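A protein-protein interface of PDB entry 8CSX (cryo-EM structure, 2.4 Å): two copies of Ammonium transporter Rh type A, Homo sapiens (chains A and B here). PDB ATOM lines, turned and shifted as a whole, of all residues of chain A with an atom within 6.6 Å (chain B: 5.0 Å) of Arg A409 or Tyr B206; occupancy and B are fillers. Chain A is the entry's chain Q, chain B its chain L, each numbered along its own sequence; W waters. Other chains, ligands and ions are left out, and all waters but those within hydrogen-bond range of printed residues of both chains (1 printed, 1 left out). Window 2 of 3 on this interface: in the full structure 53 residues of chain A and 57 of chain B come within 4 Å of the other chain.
The chain-end carboxylate (OXT) of Arg A409 lies within hydrogen-bond range of the side-chain hydroxyl (OH) of Tyr B206, 3.0 Å away.
OG of Ser B207 is in hydrogen-bond range of OH of Tyr A206 (3.0 Å).
The backbone NH (N) of Tyr A205 lies within hydrogen-bond range of the chain-end carboxylate (O) of Arg B409, 3.1 Å away.
The chain-end carboxylate (O) of Arg B409 lies within hydrogen-bond range of the backbone NH (N) of Tyr A206 (2.8 Å).
The chain-end carboxylate (OXT) of Arg B409 lies within salt-bridge range of the guanidinium group (NE) of Arg A409.
O of Lys A73 is in hydrogen-bond range of NH1 of Arg A409 (3.2 Å).
The side-chain hydroxyl of Ser A207 is in hydrogen-bond range of the guanidinium group of Arg A409, at 2.8 Å.
CB of Ala A204 touches O of Arg B409, 3.5 Å away.
OH of Tyr A206 touches CB of Ala B204 (3.6 Å).
Tyr A206 touches Tyr B206.
CD1 of Tyr A206 touches CE2 of Phe B210 (3.5 Å).
Leu A209 touches Phe B210 (CB to CE1, 3.6 Å).
Phe A210 touches Phe B210 (CZ to CZ, 3.5 Å).
Arg A409 touches just these residues of chain B: Tyr B206 (3.0 Å) and Arg B409 (2.7 Å).
Tyr B206 touches just these residues of chain A: Tyr A206 (3.5 Å) and Arg A409 (3.0 Å).
Of the printed residues of chain A, Ala B204 touches Tyr A206 (3.6 Å).
Of the printed residues of chain B, Phe A210 touches Phe B210 (3.5 Å).
Of the printed residues of chain B, Tyr A205 touches Arg B409 (3.1 Å).
Ser A203 touches none of the printed residues of chain B.
The nearest printed residue of chain B that does not touch Tyr A206 is Tyr B205 (5.1 Å).
Hydrophobic or aromatic side chains of chain B within 4 Å of the printed part of chain A: Ala B204, Tyr B206 and Phe B210.
Of the 15 printed residues of chain A, 6 touch a printed residue of chain B.
Tyr A205 touches Arg B409, but with the chains exchanged Arg A409 does not touch Tyr B205 (7.7 Å).
Tyr A206 touches Ala B204, but with the chains exchanged Ala A204 does not touch Tyr B206 (9.9 Å).
Tyr A206 touches Arg B409, and with the chains exchanged Arg A409 touches Tyr B206.
Arg A409 touches its own counterpart, Arg B409.
Positions printed for both chains: 204, 205, 206, 207, 208, 209, 210 and 409.
Of the 11 pairs that touch across the chains among the printed residues, 5 have their exchanged pair printed and touching as well.
Water W1 lies within hydrogen-bond range of N of Tyr B206 (2.7 Å), OH of Tyr A206 (3.1 Å) and N of Tyr B205 (3.2 Å).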
ATOM      1  N   LEU A  72      18.918 -21.192 -18.995  1.00  0.00           N
ATOM      2  CA  LEU A  72      17.663 -20.464 -19.137  1.00  0.00           C
ATOM      3  C   LEU A  72      16.945 -20.341 -17.797  1.00  0.00           C
ATOM      4  O   LEU A  72      16.780 -21.328 -17.076  1.00  0.00           O
ATOM      5  CB  LEU A  72      16.775 -21.159 -20.162  1.00  0.00           C
ATOM      6  CG  LEU A  72      17.267 -21.052 -21.605  1.00  0.00           C
ATOM      7  CD1 LEU A  72      16.466 -21.942 -22.535  1.00  0.00           C
ATOM      8  CD2 LEU A  72      17.224 -19.607 -22.070  1.00  0.00           C
ATOM      9  N   LYS A  73      16.498 -19.124 -17.481  1.00  0.00           N
ATOM     10  CA  LYS A  73      16.021 -18.827 -16.133  1.00  0.00           C
ATOM     11  C   LYS A  73      14.736 -19.579 -15.805  1.00  0.00           C
ATOM     12  O   LYS A  73      14.504 -19.946 -14.650  1.00  0.00           O
ATOM     13  CB  LYS A  73      15.822 -17.322 -15.969  1.00  0.00           C
ATOM     14  CG  LYS A  73      14.785 -16.738 -16.899  1.00  0.00           C
ATOM     15  CD  LYS A  73      14.517 -15.293 -16.605  1.00  0.00           C
ATOM     16  CE  LYS A  73      13.377 -14.791 -17.471  1.00  0.00           C
ATOM     17  NZ  LYS A  73      13.299 -13.312 -17.456  1.00  0.00           N
ATOM     18  N   LYS A  74      13.894 -19.829 -16.801  1.00  0.00           N
ATOM     19  CA  LYS A  74      12.633 -20.517 -16.579  1.00  0.00           C
ATOM     20  C   LYS A  74      12.554 -21.860 -17.288  1.00  0.00           C
ATOM     21  O   LYS A  74      11.451 -22.317 -17.594  1.00  0.00           O
ATOM     22  CB  LYS A  74      11.465 -19.627 -17.011  1.00  0.00           C
ATOM     23  CG  LYS A  74      11.287 -18.394 -16.159  1.00  0.00           C
ATOM     24  CD  LYS A  74      10.234 -17.472 -16.726  1.00  0.00           C
ATOM     25  CE  LYS A  74       8.864 -18.112 -16.731  1.00  0.00           C
ATOM     26  NZ  LYS A  74       8.276 -18.193 -15.365  1.00  0.00           N
ATOM     27  N   SER A 203      19.065 -15.670 -19.103  1.00  0.00           N
ATOM     28  CA  SER A 203      19.665 -16.429 -18.022  1.00  0.00           C
ATOM     29  C   SER A 203      19.468 -15.714 -16.687  1.00  0.00           C
ATOM     30  O   SER A 203      19.070 -14.553 -16.623  1.00  0.00           O
ATOM     31  CB  SER A 203      21.151 -16.663 -18.295  1.00  0.00           C
ATOM     32  OG  SER A 203      21.911 -15.512 -18.004  1.00  0.00           O
ATOM     33  N   ALA A 204      19.751 -16.438 -15.608  1.00  0.00           N
ATOM     34  CA  ALA A 204      19.810 -15.869 -14.271  1.00  0.00           C
ATOM     35  C   ALA A 204      21.125 -16.289 -13.632  1.00  0.00           C
ATOM     36  O   ALA A 204      21.865 -17.109 -14.176  1.00  0.00           O
ATOM     37  CB  ALA A 204      18.620 -16.301 -13.410  1.00  0.00           C
ATOM     38  N   TYR A 205      21.408 -15.705 -12.468  1.00  0.00           N
ATOM     39  CA  TYR A 205      22.701 -15.892 -11.818  1.00  0.00           C
ATOM     40  C   TYR A 205      22.935 -17.356 -11.440  1.00  0.00           C
ATOM     41  O   TYR A 205      23.937 -17.971 -11.841  1.00  0.00           O
ATOM     42  CB  TYR A 205      22.765 -14.978 -10.594  1.00  0.00           C
ATOM     43  CG  TYR A 205      23.994 -15.120  -9.739  1.00  0.00           C
ATOM     44  CD1 TYR A 205      25.188 -14.508 -10.098  1.00  0.00           C
ATOM     45  CD2 TYR A 205      23.959 -15.848  -8.562  1.00  0.00           C
ATOM     46  CE1 TYR A 205      26.309 -14.632  -9.317  1.00  0.00           C
ATOM     47  CE2 TYR A 205      25.074 -15.981  -7.779  1.00  0.00           C
ATOM     48  CZ  TYR A 205      26.247 -15.373  -8.159  1.00  0.00           C
ATOM     49  OH  TYR A 205      27.356 -15.496  -7.371  1.00  0.00           O
ATOM     50  N   TYR A 206      21.991 -17.949 -10.712  1.00  0.00           N
ATOM     51  CA  TYR A 206      22.165 -19.328 -10.277  1.00  0.00           C
ATOM     52  C   TYR A 206      21.961 -20.298 -11.432  1.00  0.00           C
ATOM     53  O   TYR A 206      22.556 -21.384 -11.456  1.00  0.00           O
ATOM     54  CB  TYR A 206      21.224 -19.626  -9.111  1.00  0.00           C
ATOM     55  CG  TYR A 206      21.607 -18.886  -7.849  1.00  0.00           C
ATOM     56  CD1 TYR A 206      22.810 -19.159  -7.209  1.00  0.00           C
ATOM     57  CD2 TYR A 206      20.783 -17.910  -7.305  1.00  0.00           C
ATOM     58  CE1 TYR A 206      23.176 -18.493  -6.067  1.00  0.00           C
ATOM     59  CE2 TYR A 206      21.144 -17.234  -6.157  1.00  0.00           C
ATOM     60  CZ  TYR A 206      22.343 -17.535  -5.542  1.00  0.00           C
ATOM     61  OH  TYR A 206      22.722 -16.884  -4.400  1.00  0.00           O
ATOM     62  N   SER A 207      21.146 -19.908 -12.413  1.00  0.00           N
ATOM     63  CA  SER A 207      21.043 -20.681 -13.644  1.00  0.00           C
ATOM     64  C   SER A 207      22.393 -20.770 -14.346  1.00  0.00           C
ATOM     65  O   SER A 207      22.783 -21.839 -14.825  1.00  0.00           O
ATOM     66  CB  SER A 207      19.997 -20.057 -14.566  1.00  0.00           C
ATOM     67  OG  SER A 207      18.753 -19.930 -13.912  1.00  0.00           O
ATOM     68  N   ASP A 208      23.128 -19.657 -14.393  1.00  0.00           N
ATOM     69  CA  ASP A 208      24.456 -19.670 -14.996  1.00  0.00           C
ATOM     70  C   ASP A 208      25.437 -20.498 -14.173  1.00  0.00           C
ATOM     71  O   ASP A 208      26.343 -21.125 -14.732  1.00  0.00           O
ATOM     72  CB  ASP A 208      24.971 -18.246 -15.168  1.00  0.00           C
ATOM     73  CG  ASP A 208      24.387 -17.560 -16.373  1.00  0.00           C
ATOM     74  OD1 ASP A 208      24.059 -18.252 -17.354  1.00  0.00           O
ATOM     75  OD2 ASP A 208      24.265 -16.321 -16.347  1.00  0.00           O
ATOM     76  N   LEU A 209      25.277 -20.522 -12.848  1.00  0.00           N
ATOM     77  CA  LEU A 209      26.128 -21.404 -12.048  1.00  0.00           C
ATOM     78  C   LEU A 209      25.862 -22.887 -12.345  1.00  0.00           C
ATOM     79  O   LEU A 209      26.803 -23.688 -12.457  1.00  0.00           O
ATOM     80  CB  LEU A 209      25.954 -21.091 -10.564  1.00  0.00           C
ATOM     81  CG  LEU A 209      26.579 -19.761 -10.136  1.00  0.00           C
ATOM     82  CD1 LEU A 209      26.420 -19.549  -8.651  1.00  0.00           C
ATOM     83  CD2 LEU A 209      28.049 -19.702 -10.535  1.00  0.00           C
ATOM     84  N   PHE A 210      24.589 -23.271 -12.488  1.00  0.00           N
ATOM     85  CA  PHE A 210      24.267 -24.641 -12.895  1.00  0.00           C
ATOM     86  C   PHE A 210      24.829 -24.960 -14.280  1.00  0.00           C
ATOM     87  O   PHE A 210      25.336 -26.070 -14.533  1.00  0.00           O
ATOM     88  CB  PHE A 210      22.752 -24.857 -12.893  1.00  0.00           C
ATOM     89  CG  PHE A 210      22.151 -25.028 -11.536  1.00  0.00           C
ATOM     90  CD1 PHE A 210      22.502 -26.104 -10.736  1.00  0.00           C
ATOM     91  CD2 PHE A 210      21.199 -24.134 -11.070  1.00  0.00           C
ATOM     92  CE1 PHE A 210      21.935 -26.272  -9.492  1.00  0.00           C
ATOM     93  CE2 PHE A 210      20.630 -24.295  -9.823  1.00  0.00           C
ATOM     94  CZ  PHE A 210      21.003 -25.371  -9.032  1.00  0.00           C
ATOM     95  N   PRO A 406       7.692 -24.917  -8.837  1.00  0.00           N
ATOM     96  CA  PRO A 406       7.469 -24.319  -7.519  1.00  0.00           C
ATOM     97  C   PRO A 406       7.255 -22.817  -7.615  1.00  0.00           C
ATOM     98  O   PRO A 406       7.808 -22.141  -8.483  1.00  0.00           O
ATOM     99  CB  PRO A 406       8.757 -24.646  -6.753  1.00  0.00           C
ATOM    100  CG  PRO A 406       9.413 -25.714  -7.523  1.00  0.00           C
ATOM    101  CD  PRO A 406       9.019 -25.540  -8.945  1.00  0.00           C
ATOM    102  N   LYS A 407       6.441 -22.302  -6.692  1.00  0.00           N
ATOM    103  CA  LYS A 407       6.223 -20.863  -6.600  1.00  0.00           C
ATOM    104  C   LYS A 407       7.515 -20.128  -6.279  1.00  0.00           C
ATOM    105  O   LYS A 407       7.782 -19.051  -6.823  1.00  0.00           O
ATOM    106  CB  LYS A 407       5.164 -20.567  -5.537  1.00  0.00           C
ATOM    107  CG  LYS A 407       4.916 -19.093  -5.283  1.00  0.00           C
ATOM    108  CD  LYS A 407       4.043 -18.884  -4.054  1.00  0.00           C
ATOM    109  CE  LYS A 407       2.738 -19.659  -4.161  1.00  0.00           C
ATOM    110  NZ  LYS A 407       1.893 -19.507  -2.943  1.00  0.00           N
ATOM    111  N   THR A 408       8.332 -20.700  -5.402  1.00  0.00           N
ATOM    112  CA  THR A 408       9.565 -20.075  -4.953  1.00  0.00           C
ATOM    113  C   THR A 408      10.717 -20.450  -5.878  1.00  0.00           C
ATOM    114  O   THR A 408      10.826 -21.594  -6.320  1.00  0.00           O
ATOM    115  CB  THR A 408       9.875 -20.502  -3.516  1.00  0.00           C
ATOM    116  OG1 THR A 408       8.803 -20.095  -2.659  1.00  0.00           O
ATOM    117  CG2 THR A 408      11.171 -19.888  -3.010  1.00  0.00           C
ATOM    118  N   ARG A 409      11.564 -19.474  -6.181  1.00  0.00           N
ATOM    119  CA  ARG A 409      12.776 -19.745  -6.937  1.00  0.00           C
ATOM    120  C   ARG A 409      13.942 -20.080  -6.008  1.00  0.00           C
ATOM    121  O   ARG A 409      14.523 -21.155  -6.077  1.00  0.00           O
ATOM    122  CB  ARG A 409      13.143 -18.561  -7.823  1.00  0.00           C
ATOM    123  CG  ARG A 409      14.556 -18.647  -8.353  1.00  0.00           C
ATOM    124  CD  ARG A 409      14.737 -17.899  -9.638  1.00  0.00           C
ATOM    125  NE  ARG A 409      16.071 -18.115 -10.177  1.00  0.00           N
ATOM    126  CZ  ARG A 409      16.379 -19.046 -11.068  1.00  0.00           C
ATOM    127  NH1 ARG A 409      15.459 -19.849 -11.576  1.00  0.00           N
ATOM    128  NH2 ARG A 409      17.641 -19.170 -11.464  1.00  0.00           N
ATOM    129  OXT ARG A 409      14.336 -19.279  -5.163  1.00  0.00           O
ATOM    130  N   ALA B 204      25.243 -16.053   0.407  1.00  0.00           N
ATOM    131  CA  ALA B 204      23.807 -16.143   0.238  1.00  0.00           C
ATOM    132  C   ALA B 204      23.414 -17.598   0.436  1.00  0.00           C
ATOM    133  O   ALA B 204      24.264 -18.488   0.467  1.00  0.00           O
ATOM    134  CB  ALA B 204      23.363 -15.622  -1.134  1.00  0.00           C
ATOM    135  N   TYR B 205      22.113 -17.834   0.586  1.00  0.00           N
ATOM    136  CA  TYR B 205      21.634 -19.175   0.907  1.00  0.00           C
ATOM    137  C   TYR B 205      21.968 -20.171  -0.205  1.00  0.00           C
ATOM    138  O   TYR B 205      22.599 -21.217   0.037  1.00  0.00           O
ATOM    139  CB  TYR B 205      20.130 -19.105   1.173  1.00  0.00           C
ATOM    140  CG  TYR B 205      19.539 -20.382   1.668  1.00  0.00           C
ATOM    141  CD1 TYR B 205      19.858 -20.872   2.925  1.00  0.00           C
ATOM    142  CD2 TYR B 205      18.661 -21.107   0.882  1.00  0.00           C
ATOM    143  CE1 TYR B 205      19.324 -22.046   3.378  1.00  0.00           C
ATOM    144  CE2 TYR B 205      18.122 -22.281   1.329  1.00  0.00           C
ATOM    145  CZ  TYR B 205      18.455 -22.744   2.575  1.00  0.00           C
ATOM    146  OH  TYR B 205      17.918 -23.923   3.016  1.00  0.00           O
ATOM    147  N   TYR B 206      21.600 -19.840  -1.439  1.00  0.00           N
ATOM    148  CA  TYR B 206      21.892 -20.716  -2.564  1.00  0.00           C
ATOM    149  C   TYR B 206      23.374 -20.729  -2.911  1.00  0.00           C
ATOM    150  O   TYR B 206      23.867 -21.729  -3.437  1.00  0.00           O
ATOM    151  CB  TYR B 206      21.057 -20.302  -3.769  1.00  0.00           C
ATOM    152  CG  TYR B 206      19.578 -20.488  -3.556  1.00  0.00           C
ATOM    153  CD1 TYR B 206      19.090 -21.563  -2.820  1.00  0.00           C
ATOM    154  CD2 TYR B 206      18.667 -19.594  -4.083  1.00  0.00           C
ATOM    155  CE1 TYR B 206      17.742 -21.736  -2.627  1.00  0.00           C
ATOM    156  CE2 TYR B 206      17.321 -19.762  -3.898  1.00  0.00           C
ATOM    157  CZ  TYR B 206      16.862 -20.829  -3.171  1.00  0.00           C
ATOM    158  OH  TYR B 206      15.514 -20.981  -2.985  1.00  0.00           O
ATOM    159  N   SER B 207      24.094 -19.647  -2.613  1.00  0.00           N
ATOM    160  CA  SER B 207      25.534 -19.625  -2.841  1.00  0.00           C
ATOM    161  C   SER B 207      26.249 -20.644  -1.960  1.00  0.00           C
ATOM    162  O   SER B 207      27.169 -21.332  -2.412  1.00  0.00           O
ATOM    163  CB  SER B 207      26.083 -18.219  -2.595  1.00  0.00           C
ATOM    164  OG  SER B 207      25.586 -17.293  -3.543  1.00  0.00           O
ATOM    165  N   ASP B 208      25.834 -20.759  -0.696  1.00  0.00           N
ATOM    166  CA  ASP B 208      26.397 -21.784   0.177  1.00  0.00           C
ATOM    167  C   ASP B 208      25.975 -23.177  -0.257  1.00  0.00           C
ATOM    168  O   ASP B 208      26.768 -24.126  -0.154  1.00  0.00           O
ATOM    169  CB  ASP B 208      25.984 -21.534   1.623  1.00  0.00           C
ATOM    170  CG  ASP B 208      26.762 -20.408   2.255  1.00  0.00           C
ATOM    171  OD1 ASP B 208      27.965 -20.283   1.956  1.00  0.00           O
ATOM    172  OD2 ASP B 208      26.172 -19.645   3.043  1.00  0.00           O
ATOM    173  N   LEU B 209      24.744 -23.316  -0.753  1.00  0.00           N
ATOM    174  CA  LEU B 209      24.354 -24.592  -1.346  1.00  0.00           C
ATOM    175  C   LEU B 209      25.280 -24.976  -2.501  1.00  0.00           C
ATOM    176  O   LEU B 209      25.676 -26.140  -2.625  1.00  0.00           O
ATOM    177  CB  LEU B 209      22.903 -24.524  -1.804  1.00  0.00           C
ATOM    178  CG  LEU B 209      22.298 -25.762  -2.454  1.00  0.00           C
ATOM    179  CD1 LEU B 209      22.499 -26.987  -1.583  1.00  0.00           C
ATOM    180  CD2 LEU B 209      20.832 -25.519  -2.705  1.00  0.00           C
ATOM    181  N   PHE B 210      25.647 -24.011  -3.344  1.00  0.00           N
ATOM    182  CA  PHE B 210      26.579 -24.283  -4.438  1.00  0.00           C
ATOM    183  C   PHE B 210      27.976 -24.612  -3.924  1.00  0.00           C
ATOM    184  O   PHE B 210      28.661 -25.473  -4.485  1.00  0.00           O
ATOM    185  CB  PHE B 210      26.636 -23.095  -5.395  1.00  0.00           C
ATOM    186  CG  PHE B 210      25.663 -23.181  -6.527  1.00  0.00           C
ATOM    187  CD1 PHE B 210      25.958 -23.925  -7.655  1.00  0.00           C
ATOM    188  CD2 PHE B 210      24.455 -22.506  -6.473  1.00  0.00           C
ATOM    189  CE1 PHE B 210      25.066 -24.004  -8.701  1.00  0.00           C
ATOM    190  CE2 PHE B 210      23.558 -22.579  -7.522  1.00  0.00           C
ATOM    191  CZ  PHE B 210      23.865 -23.326  -8.636  1.00  0.00           C
ATOM    192  N   ARG B 409      18.507 -13.257 -10.107  1.00  0.00           N
ATOM    193  CA  ARG B 409      19.311 -14.271  -9.431  1.00  0.00           C
ATOM    194  C   ARG B 409      18.845 -15.683  -9.780  1.00  0.00           C
ATOM    195  O   ARG B 409      19.644 -16.568 -10.084  1.00  0.00           O
ATOM    196  CB  ARG B 409      19.253 -14.079  -7.918  1.00  0.00           C
ATOM    197  CG  ARG B 409      19.552 -12.679  -7.457  1.00  0.00           C
ATOM    198  CD  ARG B 409      21.037 -12.451  -7.328  1.00  0.00           C
ATOM    199  NE  ARG B 409      21.602 -13.264  -6.260  1.00  0.00           N
ATOM    200  CZ  ARG B 409      22.896 -13.346  -5.989  1.00  0.00           C
ATOM    201  NH1 ARG B 409      23.791 -12.665  -6.684  1.00  0.00           N
ATOM    202  NH2 ARG B 409      23.302 -14.134  -5.002  1.00  0.00           N
ATOM    203  OXT ARG B 409      17.653 -15.971  -9.755  1.00  0.00           O
HETATM  204  O   HOH W   1      20.668 -17.395  -2.189  1.00  0.00           O
